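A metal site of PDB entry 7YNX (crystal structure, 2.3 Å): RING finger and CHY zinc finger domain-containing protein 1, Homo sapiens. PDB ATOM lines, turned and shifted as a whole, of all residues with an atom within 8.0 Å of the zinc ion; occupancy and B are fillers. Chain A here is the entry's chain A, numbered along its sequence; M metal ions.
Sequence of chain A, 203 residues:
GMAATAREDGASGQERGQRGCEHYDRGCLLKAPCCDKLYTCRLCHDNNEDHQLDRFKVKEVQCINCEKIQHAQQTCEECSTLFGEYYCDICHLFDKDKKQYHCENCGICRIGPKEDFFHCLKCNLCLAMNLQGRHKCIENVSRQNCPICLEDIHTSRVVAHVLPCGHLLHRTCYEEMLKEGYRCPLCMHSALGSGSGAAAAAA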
ATOM      1  N   LYS A  31      16.485  26.304 -23.040  1.00  0.00           N
ATOM      2  CA  LYS A  31      16.698  27.358 -22.045  1.00  0.00           C
ATOM      3  C   LYS A  31      15.346  28.019 -21.803  1.00  0.00           C
ATOM      4  O   LYS A  31      14.824  28.709 -22.682  1.00  0.00           O
ATOM      5  CB  LYS A  31      17.747  28.366 -22.479  1.00  0.00           C
ATOM      6  CG  LYS A  31      18.325  29.090 -21.254  1.00  0.00           C
ATOM      7  CD  LYS A  31      19.039  30.390 -21.551  1.00  0.00           C
ATOM      8  CE  LYS A  31      19.218  31.192 -20.245  1.00  0.00           C
ATOM      9  NZ  LYS A  31      20.274  32.251 -20.367  1.00  0.00           N
ATOM     10  N   ALA A  32      14.775  27.779 -20.631  1.00  0.00           N
ATOM     11  CA  ALA A  32      13.480  28.336 -20.273  1.00  0.00           C
ATOM     12  C   ALA A  32      13.572  29.849 -20.166  1.00  0.00           C
ATOM     13  O   ALA A  32      14.193  30.360 -19.222  1.00  0.00           O
ATOM     14  CB  ALA A  32      12.971  27.756 -18.955  1.00  0.00           C
ATOM     15  N   PRO A  33      12.970  30.620 -21.076  1.00  0.00           N
ATOM     16  CA  PRO A  33      13.039  32.075 -20.985  1.00  0.00           C
ATOM     17  C   PRO A  33      12.375  32.629 -19.728  1.00  0.00           C
ATOM     18  O   PRO A  33      12.519  33.834 -19.454  1.00  0.00           O
ATOM     19  CB  PRO A  33      12.313  32.539 -22.237  1.00  0.00           C
ATOM     20  CG  PRO A  33      11.330  31.441 -22.524  1.00  0.00           C
ATOM     21  CD  PRO A  33      11.957  30.156 -22.043  1.00  0.00           C
ATOM     22  N   CYS A  34      11.649  31.810 -18.964  1.00  0.00           N
ATOM     23  CA  CYS A  34      10.995  32.318 -17.745  1.00  0.00           C
ATOM     24  C   CYS A  34      11.971  32.417 -16.581  1.00  0.00           C
ATOM     25  O   CYS A  34      12.220  33.516 -16.070  1.00  0.00           O
ATOM     26  CB  CYS A  34       9.795  31.450 -17.374  1.00  0.00           C
ATOM     27  SG  CYS A  34      10.006  29.690 -17.703  1.00  0.00           S
ATOM     28  N   CYS A  35      12.528  31.278 -16.153  1.00  0.00           N
ATOM     29  CA  CYS A  35      13.463  31.238 -15.036  1.00  0.00           C
ATOM     30  C   CYS A  35      14.914  31.166 -15.496  1.00  0.00           C
ATOM     31  O   CYS A  35      15.811  30.994 -14.654  1.00  0.00           O
ATOM     32  CB  CYS A  35      13.140  30.051 -14.139  1.00  0.00           C
ATOM     33  SG  CYS A  35      13.179  28.457 -15.045  1.00  0.00           S
ATOM     34  N   ASP A  36      15.173  31.313 -16.799  1.00  0.00           N
ATOM     35  CA  ASP A  36      16.478  31.090 -17.416  1.00  0.00           C
ATOM     36  C   ASP A  36      17.224  29.902 -16.803  1.00  0.00           C
ATOM     37  O   ASP A  36      18.353  30.007 -16.334  1.00  0.00           O
ATOM     38  CB  ASP A  36      17.338  32.355 -17.414  1.00  0.00           C
ATOM     39  CG  ASP A  36      16.983  33.278 -18.570  1.00  0.00           C
ATOM     40  OD1 ASP A  36      16.581  32.761 -19.638  1.00  0.00           O
ATOM     41  OD2 ASP A  36      17.092  34.518 -18.408  1.00  0.00           O
ATOM     42  N   LYS A  37      16.530  28.765 -16.816  1.00  0.00           N
ATOM     43  CA  LYS A  37      17.097  27.483 -16.425  1.00  0.00           C
ATOM     44  C   LYS A  37      17.113  26.561 -17.642  1.00  0.00           C
ATOM     45  O   LYS A  37      16.401  26.763 -18.624  1.00  0.00           O
ATOM     46  CB  LYS A  37      16.292  26.850 -15.276  1.00  0.00           C
ATOM     47  CG  LYS A  37      16.548  27.493 -13.915  1.00  0.00           C
ATOM     48  CD  LYS A  37      15.467  27.118 -12.917  1.00  0.00           C
ATOM     49  CE  LYS A  37      16.049  26.470 -11.669  1.00  0.00           C
ATOM     50  NZ  LYS A  37      15.094  26.576 -10.529  1.00  0.00           N
ATOM     51  N   LEU A  38      17.972  25.560 -17.568  1.00  0.00           N
ATOM     52  CA  LEU A  38      18.118  24.576 -18.626  1.00  0.00           C
ATOM     53  C   LEU A  38      17.386  23.310 -18.218  1.00  0.00           C
ATOM     54  O   LEU A  38      17.747  22.670 -17.221  1.00  0.00           O
ATOM     55  CB  LEU A  38      19.584  24.274 -18.887  1.00  0.00           C
ATOM     56  CG  LEU A  38      20.364  25.430 -19.505  1.00  0.00           C
ATOM     57  CD1 LEU A  38      21.838  25.074 -19.541  1.00  0.00           C
ATOM     58  CD2 LEU A  38      19.826  25.720 -20.898  1.00  0.00           C
ATOM     59  N   TYR A  39      16.335  22.964 -18.964  1.00  0.00           N
ATOM     60  CA  TYR A  39      15.571  21.749 -18.748  1.00  0.00           C
ATOM     61  C   TYR A  39      15.550  20.960 -20.041  1.00  0.00           C
ATOM     62  O   TYR A  39      15.552  21.538 -21.141  1.00  0.00           O
ATOM     63  CB  TYR A  39      14.112  22.049 -18.307  1.00  0.00           C
ATOM     64  CG  TYR A  39      13.975  22.464 -16.858  1.00  0.00           C
ATOM     65  CD1 TYR A  39      13.965  21.509 -15.837  1.00  0.00           C
ATOM     66  CD2 TYR A  39      13.842  23.805 -16.501  1.00  0.00           C
ATOM     67  CE1 TYR A  39      13.835  21.877 -14.523  1.00  0.00           C
ATOM     68  CE2 TYR A  39      13.722  24.181 -15.176  1.00  0.00           C
ATOM     69  CZ  TYR A  39      13.716  23.217 -14.198  1.00  0.00           C
ATOM     70  OH  TYR A  39      13.598  23.585 -12.879  1.00  0.00           O
ATOM     71  N   HIS A  45      10.467  20.814 -17.247  1.00  0.00           N
ATOM     72  CA  HIS A  45      10.463  22.135 -16.624  1.00  0.00           C
ATOM     73  C   HIS A  45       9.202  22.320 -15.790  1.00  0.00           C
ATOM     74  O   HIS A  45       9.269  22.812 -14.662  1.00  0.00           O
ATOM     75  CB  HIS A  45      10.562  23.204 -17.708  1.00  0.00           C
ATOM     76  CG  HIS A  45      10.125  24.557 -17.277  1.00  0.00           C
ATOM     77  ND1 HIS A  45       8.827  24.848 -16.923  1.00  0.00           N
ATOM     78  CD2 HIS A  45      10.822  25.708 -17.149  1.00  0.00           C
ATOM     79  CE1 HIS A  45       8.743  26.119 -16.587  1.00  0.00           C
ATOM     80  NE2 HIS A  45       9.936  26.660 -16.710  1.00  0.00           N
ATOM     81  N   ASP A  46       8.054  21.928 -16.351  1.00  0.00           N
ATOM     82  CA  ASP A  46       6.778  22.183 -15.695  1.00  0.00           C
ATOM     83  C   ASP A  46       6.602  21.325 -14.459  1.00  0.00           C
ATOM     84  O   ASP A  46       5.956  21.755 -13.501  1.00  0.00           O
ATOM     85  CB  ASP A  46       5.641  21.952 -16.683  1.00  0.00           C
ATOM     86  CG  ASP A  46       5.593  23.016 -17.768  1.00  0.00           C
ATOM     87  OD1 ASP A  46       6.244  24.082 -17.622  1.00  0.00           O
ATOM     88  OD2 ASP A  46       4.891  22.789 -18.778  1.00  0.00           O
ATOM     89  N   ASN A  48       8.907  20.912 -12.407  1.00  0.00           N
ATOM     90  CA  ASN A  48       9.866  21.389 -11.407  1.00  0.00           C
ATOM     91  C   ASN A  48       9.833  22.894 -11.229  1.00  0.00           C
ATOM     92  O   ASN A  48      10.796  23.465 -10.709  1.00  0.00           O
ATOM     93  CB  ASN A  48      11.293  20.958 -11.772  1.00  0.00           C
ATOM     94  CG  ASN A  48      11.452  19.456 -11.780  1.00  0.00           C
ATOM     95  OD1 ASN A  48      11.418  18.816 -10.731  1.00  0.00           O
ATOM     96  ND2 ASN A  48      11.598  18.882 -12.970  1.00  0.00           N
ATOM     97  N   GLU A  49       8.763  23.558 -11.638  1.00  0.00           N
ATOM     98  CA  GLU A  49       8.697  24.997 -11.524  1.00  0.00           C
ATOM     99  C   GLU A  49       7.296  25.415 -11.129  1.00  0.00           C
ATOM    100  O   GLU A  49       6.307  24.825 -11.572  1.00  0.00           O
ATOM    101  CB  GLU A  49       9.108  25.662 -12.849  1.00  0.00           C
ATOM    102  CG  GLU A  49      10.590  25.498 -13.187  1.00  0.00           C
ATOM    103  CD  GLU A  49      11.519  26.118 -12.140  1.00  0.00           C
ATOM    104  OE1 GLU A  49      12.599  25.546 -11.873  1.00  0.00           O
ATOM    105  OE2 GLU A  49      11.165  27.192 -11.593  1.00  0.00           O
ATOM    106  N   ASP A  50       7.224  26.442 -10.260  1.00  0.00           N
ATOM    107  CA  ASP A  50       5.950  27.016  -9.843  1.00  0.00           C
ATOM    108  C   ASP A  50       5.057  27.317 -11.027  1.00  0.00           C
ATOM    109  O   ASP A  50       3.831  27.130 -10.962  1.00  0.00           O
ATOM    110  CB  ASP A  50       6.219  28.308  -9.066  1.00  0.00           C
ATOM    111  CG  ASP A  50       7.112  29.269  -9.847  1.00  0.00           C
ATOM    112  OD1 ASP A  50       7.998  28.779 -10.577  1.00  0.00           O
ATOM    113  OD2 ASP A  50       6.939  30.504  -9.727  1.00  0.00           O
ATOM    114  N   HIS A  51       5.645  27.766 -12.118  1.00  0.00           N
ATOM    115  CA  HIS A  51       4.956  28.268 -13.297  1.00  0.00           C
ATOM    116  C   HIS A  51       5.085  27.270 -14.437  1.00  0.00           C
ATOM    117  O   HIS A  51       5.740  26.220 -14.321  1.00  0.00           O
ATOM    118  CB  HIS A  51       5.533  29.623 -13.705  1.00  0.00           C
ATOM    119  CG  HIS A  51       7.002  29.549 -13.981  1.00  0.00           C
ATOM    120  ND1 HIS A  51       7.924  29.200 -13.017  1.00  0.00           N
ATOM    121  CD2 HIS A  51       7.708  29.737 -15.123  1.00  0.00           C
ATOM    122  CE1 HIS A  51       9.134  29.187 -13.547  1.00  0.00           C
ATOM    123  NE2 HIS A  51       9.031  29.517 -14.823  1.00  0.00           N
ATOM    124  N   GLN A  52       4.485  27.633 -15.568  1.00  0.00           N
ATOM    125  CA  GLN A  52       4.440  26.810 -16.757  1.00  0.00           C
ATOM    126  C   GLN A  52       5.332  27.428 -17.823  1.00  0.00           C
ATOM    127  O   GLN A  52       5.397  28.651 -17.927  1.00  0.00           O
ATOM    128  CB  GLN A  52       3.006  26.695 -17.272  1.00  0.00           C
ATOM    129  CG  GLN A  52       2.887  25.991 -18.609  1.00  0.00           C
ATOM    130  CD  GLN A  52       1.762  26.546 -19.433  1.00  0.00           C
ATOM    131  OE1 GLN A  52       0.784  25.852 -19.724  1.00  0.00           O
ATOM    132  NE2 GLN A  52       1.863  27.818 -19.811  1.00  0.00           N
ATOM    133  N   LEU A  53       6.022  26.577 -18.591  1.00  0.00           N
ATOM    134  CA  LEU A  53       6.949  27.040 -19.627  1.00  0.00           C
ATOM    135  C   LEU A  53       6.172  27.344 -20.918  1.00  0.00           C
ATOM    136  O   LEU A  53       5.280  26.583 -21.296  1.00  0.00           O
ATOM    137  CB  LEU A  53       8.026  25.982 -19.885  1.00  0.00           C
ATOM    138  CG  LEU A  53       9.030  26.216 -21.022  1.00  0.00           C
ATOM    139  CD1 LEU A  53       9.798  27.520 -20.795  1.00  0.00           C
ATOM    140  CD2 LEU A  53       9.977  25.057 -21.141  1.00  0.00           C
ATOM    141  N   ASP A  54       6.517  28.465 -21.564  1.00  0.00           N
ATOM    142  CA  ASP A  54       5.893  28.834 -22.851  1.00  0.00           C
ATOM    143  C   ASP A  54       6.797  28.362 -23.972  1.00  0.00           C
ATOM    144  O   ASP A  54       7.743  29.057 -24.358  1.00  0.00           O
ATOM    145  CB  ASP A  54       5.637  30.330 -22.955  1.00  0.00           C
ATOM    146  CG  ASP A  54       4.917  30.728 -24.254  1.00  0.00           C
ATOM    147  OD1 ASP A  54       4.904  29.940 -25.233  1.00  0.00           O
ATOM    148  OD2 ASP A  54       4.341  31.831 -24.323  1.00  0.00           O
HETATM  149 ZN    ZN M   1      10.883  28.549 -15.939  1.00  0.00          ZN
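A ring nitrogen (ND1) of His 51 is in hydrogen-bond range of the side-chain carboxylate (OD1) of Asp 50 (2.5 Å).
The backbone NH of Ala 32 sits at hydrogen-bond distance from the backbone carbonyl oxygen of Lys 37, 2.8 Å away.
A ring nitrogen (ND1) of His 45 lies within hydrogen-bond range of the side-chain carboxylate (OD1) of Asp 46 (2.8 Å).
The zinc ion is bound by a ring nitrogen (NE2) of His 45, the side-chain sulfur (SG) of Cys 34, a ring nitrogen (NE2) of His 51 and the side-chain sulfur (SG) of Cys 35.
Merely in contact with the zinc ion: Ala 32 (3.8 Å).
Five residues have an atom within 4 Å of the zinc ion: Ala 32, Cys 34, Cys 35, His 45 and His 51.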
